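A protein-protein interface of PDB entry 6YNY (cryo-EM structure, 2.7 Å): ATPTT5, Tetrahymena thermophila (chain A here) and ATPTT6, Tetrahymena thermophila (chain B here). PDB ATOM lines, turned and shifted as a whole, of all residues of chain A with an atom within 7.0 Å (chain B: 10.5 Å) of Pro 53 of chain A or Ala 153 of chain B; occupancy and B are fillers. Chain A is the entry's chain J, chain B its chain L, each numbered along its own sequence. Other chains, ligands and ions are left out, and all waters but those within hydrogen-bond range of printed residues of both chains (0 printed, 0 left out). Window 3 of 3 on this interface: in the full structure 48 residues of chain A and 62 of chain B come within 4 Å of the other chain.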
ATOM      1  N   GLY A   8      19.873 -27.466  17.021  1.00  0.00           N
ATOM      2  CA  GLY A   8      20.187 -26.865  18.300  1.00  0.00           C
ATOM      3  C   GLY A   8      19.184 -25.788  18.676  1.00  0.00           C
ATOM      4  O   GLY A   8      18.698 -25.036  17.832  1.00  0.00           O
ATOM      5  N   GLN A   9      18.877 -25.724  19.966  1.00  0.00           N
ATOM      6  CA  GLN A   9      17.935 -24.762  20.512  1.00  0.00           C
ATOM      7  C   GLN A   9      18.656 -23.821  21.461  1.00  0.00           C
ATOM      8  O   GLN A   9      19.568 -24.228  22.184  1.00  0.00           O
ATOM      9  CB  GLN A   9      16.792 -25.461  21.242  1.00  0.00           C
ATOM     10  CG  GLN A   9      15.967 -26.365  20.359  1.00  0.00           C
ATOM     11  CD  GLN A   9      15.280 -25.617  19.244  1.00  0.00           C
ATOM     12  OE1 GLN A   9      15.094 -24.403  19.315  1.00  0.00           O
ATOM     13  NE2 GLN A   9      14.904 -26.337  18.201  1.00  0.00           N
ATOM     14  N   ILE A  10      18.242 -22.557  21.450  1.00  0.00           N
ATOM     15  CA  ILE A  10      18.854 -21.535  22.286  1.00  0.00           C
ATOM     16  C   ILE A  10      18.278 -21.614  23.692  1.00  0.00           C
ATOM     17  O   ILE A  10      17.268 -22.286  23.928  1.00  0.00           O
ATOM     18  CB  ILE A  10      18.662 -20.131  21.688  1.00  0.00           C
ATOM     19  CG1 ILE A  10      17.181 -19.779  21.584  1.00  0.00           C
ATOM     20  CG2 ILE A  10      19.296 -20.065  20.328  1.00  0.00           C
ATOM     21  CD1 ILE A  10      16.934 -18.320  21.376  1.00  0.00           C
ATOM     22  N   ALA A  12      16.631 -19.521  25.347  1.00  0.00           N
ATOM     23  CA  ALA A  12      15.293 -18.968  25.479  1.00  0.00           C
ATOM     24  C   ALA A  12      14.212 -20.005  25.218  1.00  0.00           C
ATOM     25  O   ALA A  12      13.079 -19.834  25.677  1.00  0.00           O
ATOM     26  CB  ALA A  12      15.120 -17.788  24.530  1.00  0.00           C
ATOM     27  N   TYR A  13      14.531 -21.071  24.484  1.00  0.00           N
ATOM     28  CA  TYR A  13      13.535 -22.100  24.216  1.00  0.00           C
ATOM     29  C   TYR A  13      13.193 -22.890  25.469  1.00  0.00           C
ATOM     30  O   TYR A  13      12.076 -23.402  25.589  1.00  0.00           O
ATOM     31  CB  TYR A  13      14.032 -23.039  23.123  1.00  0.00           C
ATOM     32  CG  TYR A  13      13.060 -24.141  22.790  1.00  0.00           C
ATOM     33  CD1 TYR A  13      11.897 -23.872  22.094  1.00  0.00           C
ATOM     34  CD2 TYR A  13      13.305 -25.448  23.170  1.00  0.00           C
ATOM     35  CE1 TYR A  13      11.006 -24.867  21.788  1.00  0.00           C
ATOM     36  CE2 TYR A  13      12.419 -26.453  22.867  1.00  0.00           C
ATOM     37  CZ  TYR A  13      11.269 -26.156  22.175  1.00  0.00           C
ATOM     38  OH  TYR A  13      10.377 -27.155  21.868  1.00  0.00           O
ATOM     39  N   HIS A  19       8.280 -22.576  20.434  1.00  0.00           N
ATOM     40  CA  HIS A  19       8.743 -21.622  19.441  1.00  0.00           C
ATOM     41  C   HIS A  19       7.687 -20.592  19.079  1.00  0.00           C
ATOM     42  O   HIS A  19       7.990 -19.651  18.339  1.00  0.00           O
ATOM     43  CB  HIS A  19       9.172 -22.338  18.159  1.00  0.00           C
ATOM     44  CG  HIS A  19      10.348 -23.244  18.329  1.00  0.00           C
ATOM     45  ND1 HIS A  19      10.254 -24.612  18.199  1.00  0.00           N
ATOM     46  CD2 HIS A  19      11.644 -22.980  18.608  1.00  0.00           C
ATOM     47  CE1 HIS A  19      11.442 -25.151  18.395  1.00  0.00           C
ATOM     48  NE2 HIS A  19      12.303 -24.183  18.646  1.00  0.00           N
ATOM     49  N   ARG A  50       7.088 -18.124  14.117  1.00  0.00           N
ATOM     50  CA  ARG A  50       7.936 -18.281  15.284  1.00  0.00           C
ATOM     51  C   ARG A  50       8.462 -16.940  15.770  1.00  0.00           C
ATOM     52  O   ARG A  50       8.699 -16.015  14.989  1.00  0.00           O
ATOM     53  CB  ARG A  50       9.116 -19.196  14.968  1.00  0.00           C
ATOM     54  CG  ARG A  50       8.730 -20.601  14.622  1.00  0.00           C
ATOM     55  CD  ARG A  50       9.938 -21.501  14.573  1.00  0.00           C
ATOM     56  NE  ARG A  50       9.578 -22.880  14.278  1.00  0.00           N
ATOM     57  CZ  ARG A  50      10.408 -23.906  14.398  1.00  0.00           C
ATOM     58  NH1 ARG A  50      11.651 -23.717  14.812  1.00  0.00           N
ATOM     59  NH2 ARG A  50       9.992 -25.126  14.106  1.00  0.00           N
ATOM     60  N   GLN A  51       8.644 -16.847  17.083  1.00  0.00           N
ATOM     61  CA  GLN A  51       9.280 -15.705  17.710  1.00  0.00           C
ATOM     62  C   GLN A  51      10.476 -16.110  18.554  1.00  0.00           C
ATOM     63  O   GLN A  51      11.127 -15.241  19.143  1.00  0.00           O
ATOM     64  CB  GLN A  51       8.266 -14.939  18.565  1.00  0.00           C
ATOM     65  CG  GLN A  51       7.170 -14.295  17.749  1.00  0.00           C
ATOM     66  CD  GLN A  51       6.135 -13.597  18.588  1.00  0.00           C
ATOM     67  OE1 GLN A  51       5.086 -14.155  18.889  1.00  0.00           O
ATOM     68  NE2 GLN A  51       6.412 -12.357  18.949  1.00  0.00           N
ATOM     69  N   VAL A  52      10.783 -17.400  18.626  1.00  0.00           N
ATOM     70  CA  VAL A  52      11.964 -17.904  19.317  1.00  0.00           C
ATOM     71  C   VAL A  52      12.870 -18.541  18.271  1.00  0.00           C
ATOM     72  O   VAL A  52      12.508 -19.574  17.691  1.00  0.00           O
ATOM     73  CB  VAL A  52      11.589 -18.905  20.418  1.00  0.00           C
ATOM     74  CG1 VAL A  52      12.823 -19.364  21.147  1.00  0.00           C
ATOM     75  CG2 VAL A  52      10.608 -18.286  21.387  1.00  0.00           C
ATOM     76  N   PRO A  53      14.039 -17.974  17.990  1.00  0.00           N
ATOM     77  CA  PRO A  53      14.870 -18.507  16.910  1.00  0.00           C
ATOM     78  C   PRO A  53      15.515 -19.830  17.284  1.00  0.00           C
ATOM     79  O   PRO A  53      15.588 -20.221  18.450  1.00  0.00           O
ATOM     80  CB  PRO A  53      15.918 -17.416  16.704  1.00  0.00           C
ATOM     81  CG  PRO A  53      16.025 -16.764  18.009  1.00  0.00           C
ATOM     82  CD  PRO A  53      14.669 -16.810  18.629  1.00  0.00           C
ATOM     83  N   SER A  54      15.988 -20.524  16.254  1.00  0.00           N
ATOM     84  CA  SER A  54      16.607 -21.828  16.414  1.00  0.00           C
ATOM     85  C   SER A  54      17.688 -21.992  15.356  1.00  0.00           C
ATOM     86  O   SER A  54      17.871 -21.138  14.486  1.00  0.00           O
ATOM     87  CB  SER A  54      15.561 -22.937  16.322  1.00  0.00           C
ATOM     88  OG  SER A  54      16.148 -24.212  16.489  1.00  0.00           O
ATOM     89  N   GLN A  55      18.409 -23.108  15.443  1.00  0.00           N
ATOM     90  CA  GLN A  55      19.467 -23.386  14.482  1.00  0.00           C
ATOM     91  C   GLN A  55      18.909 -23.672  13.096  1.00  0.00           C
ATOM     92  O   GLN A  55      19.581 -23.412  12.094  1.00  0.00           O
ATOM     93  CB  GLN A  55      20.302 -24.567  14.964  1.00  0.00           C
ATOM     94  CG  GLN A  55      21.513 -24.873  14.114  1.00  0.00           C
ATOM     95  CD  GLN A  55      22.280 -26.073  14.611  1.00  0.00           C
ATOM     96  OE1 GLN A  55      21.719 -26.969  15.236  1.00  0.00           O
ATOM     97  NE2 GLN A  55      23.573 -26.094  14.344  1.00  0.00           N
ATOM     98  N   ASP A  56      17.691 -24.203  13.020  1.00  0.00           N
ATOM     99  CA  ASP A  56      17.097 -24.597  11.753  1.00  0.00           C
ATOM    100  C   ASP A  56      16.143 -23.560  11.184  1.00  0.00           C
ATOM    101  O   ASP A  56      15.892 -23.574   9.975  1.00  0.00           O
ATOM    102  CB  ASP A  56      16.342 -25.919  11.914  1.00  0.00           C
ATOM    103  CG  ASP A  56      15.180 -25.814  12.874  1.00  0.00           C
ATOM    104  OD1 ASP A  56      15.312 -25.113  13.898  1.00  0.00           O
ATOM    105  OD2 ASP A  56      14.129 -26.428  12.603  1.00  0.00           O
ATOM    106  N   ARG A  57      15.611 -22.668  12.014  1.00  0.00           N
ATOM    107  CA  ARG A  57      14.599 -21.718  11.582  1.00  0.00           C
ATOM    108  C   ARG A  57      14.828 -20.382  12.262  1.00  0.00           C
ATOM    109  O   ARG A  57      14.993 -20.323  13.483  1.00  0.00           O
ATOM    110  CB  ARG A  57      13.195 -22.230  11.903  1.00  0.00           C
ATOM    111  CG  ARG A  57      12.779 -23.446  11.115  1.00  0.00           C
ATOM    112  CD  ARG A  57      12.501 -23.104   9.674  1.00  0.00           C
ATOM    113  NE  ARG A  57      12.068 -24.267   8.911  1.00  0.00           N
ATOM    114  CZ  ARG A  57      12.889 -25.130   8.326  1.00  0.00           C
ATOM    115  NH1 ARG A  57      14.199 -24.979   8.408  1.00  0.00           N
ATOM    116  NH2 ARG A  57      12.393 -26.151   7.652  1.00  0.00           N
ATOM    117  N   ALA A  58      14.838 -19.316  11.470  1.00  0.00           N
ATOM    118  CA  ALA A  58      14.865 -17.974  12.018  1.00  0.00           C
ATOM    119  C   ALA A  58      13.507 -17.640  12.626  1.00  0.00           C
ATOM    120  O   ALA A  58      12.547 -18.409  12.536  1.00  0.00           O
ATOM    121  CB  ALA A  58      15.246 -16.972  10.936  1.00  0.00           C
ATOM    122  N   ALA A  59      13.423 -16.472  13.254  1.00  0.00           N
ATOM    123  CA  ALA A  59      12.219 -16.077  13.962  1.00  0.00           C
ATOM    124  C   ALA A  59      11.947 -14.598  13.748  1.00  0.00           C
ATOM    125  O   ALA A  59      12.806 -13.838  13.298  1.00  0.00           O
ATOM    126  CB  ALA A  59      12.336 -16.368  15.456  1.00  0.00           C
ATOM    127  N   PHE A  60      10.727 -14.204  14.084  1.00  0.00           N
ATOM    128  CA  PHE A  60      10.318 -12.814  14.057  1.00  0.00           C
ATOM    129  C   PHE A  60      10.501 -12.189  15.431  1.00  0.00           C
ATOM    130  O   PHE A  60      10.641 -12.877  16.443  1.00  0.00           O
ATOM    131  CB  PHE A  60       8.860 -12.684  13.629  1.00  0.00           C
ATOM    132  CG  PHE A  60       8.601 -13.086  12.218  1.00  0.00           C
ATOM    133  CD1 PHE A  60       8.767 -12.188  11.189  1.00  0.00           C
ATOM    134  CD2 PHE A  60       8.174 -14.361  11.919  1.00  0.00           C
ATOM    135  CE1 PHE A  60       8.522 -12.555   9.895  1.00  0.00           C
ATOM    136  CE2 PHE A  60       7.930 -14.728  10.627  1.00  0.00           C
ATOM    137  CZ  PHE A  60       8.104 -13.826   9.614  1.00  0.00           C
ATOM    138  N   GLY A  61      10.499 -10.865  15.456  1.00  0.00           N
ATOM    139  CA  GLY A  61      10.602 -10.114  16.685  1.00  0.00           C
ATOM    140  C   GLY A  61       9.260  -9.924  17.352  1.00  0.00           C
ATOM    141  O   GLY A  61       8.279 -10.606  17.051  1.00  0.00           O
ATOM    142  N   LEU A  62       9.222  -8.970  18.274  1.00  0.00           N
ATOM    143  CA  LEU A  62       7.992  -8.681  18.992  1.00  0.00           C
ATOM    144  C   LEU A  62       6.989  -8.010  18.065  1.00  0.00           C
ATOM    145  O   LEU A  62       7.347  -7.180  17.227  1.00  0.00           O
ATOM    146  CB  LEU A  62       8.278  -7.791  20.197  1.00  0.00           C
ATOM    147  CG  LEU A  62       9.296  -8.332  21.197  1.00  0.00           C
ATOM    148  CD1 LEU A  62       9.510  -7.337  22.307  1.00  0.00           C
ATOM    149  CD2 LEU A  62       8.857  -9.653  21.760  1.00  0.00           C
ATOM    150  N   TYR B  83      24.180 -25.069  25.342  1.00  0.00           N
ATOM    151  CA  TYR B  83      23.757 -23.802  24.768  1.00  0.00           C
ATOM    152  C   TYR B  83      24.862 -23.053  24.039  1.00  0.00           C
ATOM    153  O   TYR B  83      24.556 -22.144  23.260  1.00  0.00           O
ATOM    154  CB  TYR B  83      23.190 -22.891  25.859  1.00  0.00           C
ATOM    155  CG  TYR B  83      22.095 -23.526  26.675  1.00  0.00           C
ATOM    156  CD1 TYR B  83      20.864 -23.803  26.114  1.00  0.00           C
ATOM    157  CD2 TYR B  83      22.291 -23.840  28.008  1.00  0.00           C
ATOM    158  CE1 TYR B  83      19.863 -24.378  26.849  1.00  0.00           C
ATOM    159  CE2 TYR B  83      21.291 -24.418  28.754  1.00  0.00           C
ATOM    160  CZ  TYR B  83      20.077 -24.684  28.169  1.00  0.00           C
ATOM    161  OH  TYR B  83      19.072 -25.261  28.904  1.00  0.00           O
ATOM    162  N   ILE B  86      26.909 -25.647  20.257  1.00  0.00           N
ATOM    163  CA  ILE B  86      25.929 -26.286  19.375  1.00  0.00           C
ATOM    164  C   ILE B  86      26.647 -26.801  18.130  1.00  0.00           C
ATOM    165  O   ILE B  86      27.367 -26.029  17.474  1.00  0.00           O
ATOM    166  CB  ILE B  86      24.822 -25.300  19.011  1.00  0.00           C
ATOM    167  CG1 ILE B  86      24.085 -24.866  20.279  1.00  0.00           C
ATOM    168  CG2 ILE B  86      23.860 -25.924  18.031  1.00  0.00           C
ATOM    169  CD1 ILE B  86      22.994 -23.863  20.055  1.00  0.00           C
ATOM    170  N   ARG B  94      16.974 -21.547   7.060  1.00  0.00           N
ATOM    171  CA  ARG B  94      16.508 -20.734   8.177  1.00  0.00           C
ATOM    172  C   ARG B  94      15.473 -19.710   7.738  1.00  0.00           C
ATOM    173  O   ARG B  94      14.508 -19.445   8.464  1.00  0.00           O
ATOM    174  CB  ARG B  94      17.691 -20.035   8.834  1.00  0.00           C
ATOM    175  CG  ARG B  94      18.564 -20.945   9.652  1.00  0.00           C
ATOM    176  CD  ARG B  94      19.760 -20.221  10.210  1.00  0.00           C
ATOM    177  NE  ARG B  94      19.404 -18.951  10.832  1.00  0.00           N
ATOM    178  CZ  ARG B  94      18.859 -18.838  12.035  1.00  0.00           C
ATOM    179  NH1 ARG B  94      18.596 -19.913  12.749  1.00  0.00           N
ATOM    180  NH2 ARG B  94      18.571 -17.646  12.522  1.00  0.00           N
ATOM    181  N   ASN B  95      15.650 -19.125   6.562  1.00  0.00           N
ATOM    182  CA  ASN B  95      14.774 -18.066   6.089  1.00  0.00           C
ATOM    183  C   ASN B  95      13.437 -18.580   5.583  1.00  0.00           C
ATOM    184  O   ASN B  95      12.668 -17.800   5.016  1.00  0.00           O
ATOM    185  CB  ASN B  95      15.474 -17.261   4.997  1.00  0.00           C
ATOM    186  CG  ASN B  95      16.628 -16.446   5.528  1.00  0.00           C
ATOM    187  OD1 ASN B  95      17.022 -16.584   6.686  1.00  0.00           O
ATOM    188  ND2 ASN B  95      17.184 -15.591   4.683  1.00  0.00           N
ATOM    189  N   THR B  97      11.075 -19.337   7.499  1.00  0.00           N
ATOM    190  CA  THR B  97      10.111 -18.661   8.357  1.00  0.00           C
ATOM    191  C   THR B  97       9.615 -17.369   7.724  1.00  0.00           C
ATOM    192  O   THR B  97       8.422 -17.054   7.793  1.00  0.00           O
ATOM    193  CB  THR B  97      10.745 -18.384   9.717  1.00  0.00           C
ATOM    194  OG1 THR B  97      11.041 -19.622  10.371  1.00  0.00           O
ATOM    195  CG2 THR B  97       9.820 -17.572  10.580  1.00  0.00           C
ATOM    196  N   TYR B  98      10.516 -16.610   7.102  1.00  0.00           N
ATOM    197  CA  TYR B  98      10.125 -15.368   6.449  1.00  0.00           C
ATOM    198  C   TYR B  98       9.427 -15.625   5.120  1.00  0.00           C
ATOM    199  O   TYR B  98       8.509 -14.888   4.748  1.00  0.00           O
ATOM    200  CB  TYR B  98      11.353 -14.488   6.239  1.00  0.00           C
ATOM    201  CG  TYR B  98      12.183 -14.283   7.478  1.00  0.00           C
ATOM    202  CD1 TYR B  98      11.599 -13.896   8.671  1.00  0.00           C
ATOM    203  CD2 TYR B  98      13.549 -14.491   7.460  1.00  0.00           C
ATOM    204  CE1 TYR B  98      12.351 -13.715   9.800  1.00  0.00           C
ATOM    205  CE2 TYR B  98      14.309 -14.311   8.586  1.00  0.00           C
ATOM    206  CZ  TYR B  98      13.708 -13.924   9.754  1.00  0.00           C
ATOM    207  OH  TYR B  98      14.469 -13.745  10.879  1.00  0.00           O
ATOM    208  N   ILE B 150      10.814  -5.478   8.297  1.00  0.00           N
ATOM    209  CA  ILE B 150      10.479  -6.621   9.136  1.00  0.00           C
ATOM    210  C   ILE B 150      11.466  -6.665  10.290  1.00  0.00           C
ATOM    211  O   ILE B 150      12.681  -6.712  10.069  1.00  0.00           O
ATOM    212  CB  ILE B 150      10.518  -7.945   8.356  1.00  0.00           C
ATOM    213  CG1 ILE B 150       9.546  -7.920   7.181  1.00  0.00           C
ATOM    214  CG2 ILE B 150      10.201  -9.101   9.272  1.00  0.00           C
ATOM    215  CD1 ILE B 150       8.118  -7.747   7.568  1.00  0.00           C
ATOM    216  N   VAL B 151      10.951  -6.647  11.512  1.00  0.00           N
ATOM    217  CA  VAL B 151      11.776  -6.806  12.702  1.00  0.00           C
ATOM    218  C   VAL B 151      11.901  -8.293  12.991  1.00  0.00           C
ATOM    219  O   VAL B 151      10.895  -8.989  13.162  1.00  0.00           O
ATOM    220  CB  VAL B 151      11.184  -6.058  13.903  1.00  0.00           C
ATOM    221  CG1 VAL B 151      12.068  -6.228  15.115  1.00  0.00           C
ATOM    222  CG2 VAL B 151      11.034  -4.602  13.582  1.00  0.00           C
ATOM    223  N   ALA B 152      13.133  -8.777  13.043  1.00  0.00           N
ATOM    224  CA  ALA B 152      13.419 -10.184  13.239  1.00  0.00           C
ATOM    225  C   ALA B 152      14.143 -10.385  14.561  1.00  0.00           C
ATOM    226  O   ALA B 152      14.643  -9.444  15.179  1.00  0.00           O
ATOM    227  CB  ALA B 152      14.254 -10.738  12.084  1.00  0.00           C
ATOM    228  N   ALA B 153      14.185 -11.639  14.990  1.00  0.00           N
ATOM    229  CA  ALA B 153      14.827 -11.994  16.242  1.00  0.00           C
ATOM    230  C   ALA B 153      16.341 -12.006  16.089  1.00  0.00           C
ATOM    231  O   ALA B 153      16.881 -12.339  15.031  1.00  0.00           O
ATOM    232  CB  ALA B 153      14.347 -13.361  16.718  1.00  0.00           C
ATOM    233  N   ALA B 154      17.021 -11.642  17.168  1.00  0.00           N
ATOM    234  CA  ALA B 154      18.476 -11.600  17.198  1.00  0.00           C
ATOM    235  C   ALA B 154      19.005 -12.930  17.711  1.00  0.00           C
ATOM    236  O   ALA B 154      18.679 -13.347  18.826  1.00  0.00           O
ATOM    237  CB  ALA B 154      18.960 -10.451  18.077  1.00  0.00           C
ATOM    238  N   ASP B 155      19.820 -13.593  16.900  1.00  0.00           N
ATOM    239  CA  ASP B 155      20.381 -14.883  17.255  1.00  0.00           C
ATOM    240  C   ASP B 155      21.820 -14.945  16.768  1.00  0.00           C
ATOM    241  O   ASP B 155      22.280 -14.093  16.005  1.00  0.00           O
ATOM    242  CB  ASP B 155      19.552 -16.031  16.674  1.00  0.00           C
ATOM    243  CG  ASP B 155      19.398 -15.938  15.176  1.00  0.00           C
ATOM    244  OD1 ASP B 155      20.396 -16.150  14.461  1.00  0.00           O
ATOM    245  OD2 ASP B 155      18.277 -15.658  14.712  1.00  0.00           O
ATOM    246  N   ARG B 156      22.536 -15.973  17.222  1.00  0.00           N
ATOM    247  CA  ARG B 156      23.932 -16.138  16.849  1.00  0.00           C
ATOM    248  C   ARG B 156      24.117 -16.395  15.363  1.00  0.00           C
ATOM    249  O   ARG B 156      25.248 -16.309  14.874  1.00  0.00           O
ATOM    250  CB  ARG B 156      24.549 -17.289  17.637  1.00  0.00           C
ATOM    251  CG  ARG B 156      24.011 -18.643  17.254  1.00  0.00           C
ATOM    252  CD  ARG B 156      24.509 -19.713  18.188  1.00  0.00           C
ATOM    253  NE  ARG B 156      23.942 -19.578  19.521  1.00  0.00           N
ATOM    254  CZ  ARG B 156      24.306 -20.313  20.562  1.00  0.00           C
ATOM    255  NH1 ARG B 156      23.734 -20.120  21.737  1.00  0.00           N
ATOM    256  NH2 ARG B 156      25.247 -21.236  20.431  1.00  0.00           N
ATOM    257  N   TRP B 157      23.047 -16.711  14.640  1.00  0.00           N
ATOM    258  CA  TRP B 157      23.122 -17.029  13.225  1.00  0.00           C
ATOM    259  C   TRP B 157      22.756 -15.849  12.340  1.00  0.00           C
ATOM    260  O   TRP B 157      22.590 -16.024  11.131  1.00  0.00           O
ATOM    261  CB  TRP B 157      22.224 -18.221  12.918  1.00  0.00           C
ATOM    262  CG  TRP B 157      22.599 -19.443  13.677  1.00  0.00           C
ATOM    263  CD1 TRP B 157      23.615 -20.299  13.396  1.00  0.00           C
ATOM    264  CD2 TRP B 157      21.961 -19.949  14.853  1.00  0.00           C
ATOM    265  NE1 TRP B 157      23.654 -21.307  14.322  1.00  0.00           N
ATOM    266  CE2 TRP B 157      22.647 -21.116  15.227  1.00  0.00           C
ATOM    267  CE3 TRP B 157      20.877 -19.529  15.625  1.00  0.00           C
ATOM    268  CZ2 TRP B 157      22.286 -21.866  16.335  1.00  0.00           C
ATOM    269  CZ3 TRP B 157      20.523 -20.273  16.721  1.00  0.00           C
ATOM    270  CH2 TRP B 157      21.223 -21.428  17.069  1.00  0.00           C
ATOM    271  N   ASN B 158      22.616 -14.658  12.912  1.00  0.00           N
ATOM    272  CA  ASN B 158      22.444 -13.461  12.106  1.00  0.00           C
ATOM    273  C   ASN B 158      23.719 -13.183  11.323  1.00  0.00           C
ATOM    274  O   ASN B 158      24.804 -13.081  11.901  1.00  0.00           O
ATOM    275  CB  ASN B 158      22.108 -12.261  12.989  1.00  0.00           C
ATOM    276  CG  ASN B 158      20.879 -12.477  13.840  1.00  0.00           C
ATOM    277  OD1 ASN B 158      20.866 -12.138  15.020  1.00  0.00           O
ATOM    278  ND2 ASN B 158      19.840 -13.037  13.250  1.00  0.00           N
ATOM    279  N   HIS B 159      23.589 -13.062  10.005  1.00  0.00           N
ATOM    280  CA  HIS B 159      24.721 -12.741   9.141  1.00  0.00           C
ATOM    281  C   HIS B 159      25.847 -13.762   9.286  1.00  0.00           C
ATOM    282  O   HIS B 159      27.028 -13.416   9.243  1.00  0.00           O
ATOM    283  CB  HIS B 159      25.248 -11.336   9.433  1.00  0.00           C
ATOM    284  CG  HIS B 159      24.327 -10.233   9.021  1.00  0.00           C
ATOM    285  ND1 HIS B 159      23.637  -9.466   9.931  1.00  0.00           N
ATOM    286  CD2 HIS B 159      24.004  -9.751   7.800  1.00  0.00           C
ATOM    287  CE1 HIS B 159      22.918  -8.565   9.288  1.00  0.00           C
ATOM    288  NE2 HIS B 159      23.122  -8.717   7.993  1.00  0.00           N
ATOM    289  N   ARG B 163      30.211 -13.164   8.183  1.00  0.00           N
ATOM    290  CA  ARG B 163      31.049 -12.731   9.294  1.00  0.00           C
ATOM    291  C   ARG B 163      32.503 -12.578   8.879  1.00  0.00           C
ATOM    292  O   ARG B 163      33.250 -11.848   9.538  1.00  0.00           O
ATOM    293  CB  ARG B 163      30.949 -13.715  10.458  1.00  0.00           C
ATOM    294  CG  ARG B 163      29.554 -13.941  10.989  1.00  0.00           C
ATOM    295  CD  ARG B 163      28.906 -12.653  11.427  1.00  0.00           C
ATOM    296  NE  ARG B 163      27.623 -12.870  12.082  1.00  0.00           N
ATOM    297  CZ  ARG B 163      27.468 -13.064  13.386  1.00  0.00           C
ATOM    298  NH1 ARG B 163      26.259 -13.252  13.883  1.00  0.00           N
ATOM    299  NH2 ARG B 163      28.509 -13.065  14.198  1.00  0.00           N
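The backbone NH (N) of Ala 58 of chain A is in hydrogen-bond range of the backbone carbonyl oxygen (O) of Arg 94 of chain B, at 3.0 Å.
OG1 of Thr 97 of chain B sits at hydrogen-bond distance from O of Ala 58 of chain A (2.9 Å).
The side-chain hydroxyl (OH) of Tyr 98 of chain B is in hydrogen-bond range of the backbone carbonyl oxygen (O) of Ala 59 of chain A, 2.9 Å away.
The backbone carbonyl oxygen of Ala 59 of chain A is in hydrogen-bond range of the backbone NH of Ala 153 of chain B (3.1 Å).
The backbone NH (N) of Gly 61 of chain A sits at hydrogen-bond distance from the backbone carbonyl oxygen (O) of Val 151 of chain B (3.0 Å).
The backbone carbonyl oxygen (O) of Ser 54 of chain A lies close to the guanidinium group (NH1) of Arg 94 of chain B (2.2 Å).
The side-chain hydroxyl (OG) of Ser 54 of chain A sits at hydrogen-bond distance from the backbone carbonyl oxygen (O) of Gly 8 of chain A (3.0 Å).
The side-chain amide nitrogen (NE2) of Gln 9 of chain A lies within hydrogen-bond range of the side-chain hydroxyl (OG) of Ser 54 of chain A (3.0 Å).
The backbone carbonyl oxygen (O) of Arg 50 of chain A lies within hydrogen-bond range of the backbone NH (N) of Phe 60 of chain A (2.9 Å).
The side-chain hydroxyl of Ser 54 of chain A lies within hydrogen-bond range of the side-chain carboxylate of Asp 56 of chain A, 2.9 Å away.
The guanidinium group (NH2) of Arg 94 of chain B lies within salt-bridge range of the side-chain carboxylate (OD2) of Asp 155 of chain B, at 3.0 Å.
The side-chain carboxylate (OD1) of Asp 155 of chain B lies within hydrogen-bond range of the backbone NH (N) of Trp 157 of chain B, at 2.7 Å.
Among the printed residues, pairs that only touch across the chains: Gly 8 of chain A with Ile 86 of chain B, Ile 10 of chain A with Trp 157 of chain B, Pro 53 of chain A with Ala 153 of chain B, Pro 53 of chain A with Asp 155 of chain B, Ser 54 of chain A with Trp 157 of chain B, Gln 55 of chain A with Ile 86 of chain B, Gln 55 of chain A with Arg 94 of chain B, Gln 55 of chain A with Trp 157 of chain B, Asp 56 of chain A with Arg 94 of chain B, Arg 57 of chain A with Arg 94 of chain B, Arg 57 of chain A with Thr 97 of chain B, Ala 58 of chain A with Tyr 98 of chain B, Ala 59 of chain A with Ala 152 of chain B, Phe 60 of chain A with Thr 97 of chain B, Phe 60 of chain A with Tyr 98 of chain B, Phe 60 of chain A with Ile 150 of chain B, Phe 60 of chain A with Val 151 of chain B, Phe 60 of chain A with Ala 153 of chain B, Gly 61 of chain A with Ala 152 of chain B and Gly 61 of chain A with Ala 153 of chain B.
Pro 53 of chain A touches just these residues of chain B: Ala 153 and Asp 155.
Of the printed residues of chain B, Gln 55 of chain A touches Ile 86 (3.7 Å), Arg 94 (3.6 Å) and Trp 157 (3.6 Å).
Of chain B, only Val 151 (3.0 Å), Ala 152 (3.7 Å) and Ala 153 (3.8 Å) come within 4 Å of Gly 61 of chain A.
Tyr 83 of chain B touches none of the printed residues of chain A.
Printed residues of chain A within 4 Å of Ile 86 of chain B: Gly 8 and Gln 55.
Of the printed residues of chain A, Tyr 98 of chain B touches Ala 58, Ala 59 and Phe 60.
Of the printed residues of chain A, Asp 155 of chain B touches Pro 53 (3.6 Å).
Arg 163 of chain B touches none of the printed residues of chain A.
Of the 19 printed residues of chain A, 11 touch a printed residue of chain B.
Printed residues of chain A that touch a printed residue of chain B: Gly 8, Ile 10, Pro 53, Ser 54, Gln 55, Asp 56, Arg 57, Ala 58, Ala 59, Phe 60 and Gly 61.
Hydrophobic or aromatic side chains of chain A that line the printed part of chain B: Ile 10, Pro 53, Ala 58, Ala 59 and Phe 60.
Hydrophobic or aromatic side chains of chain B within 4 Å of the printed part of chain A: Ile 86, Tyr 98, Ile 150, Ala 152, Ala 153 and Trp 157.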
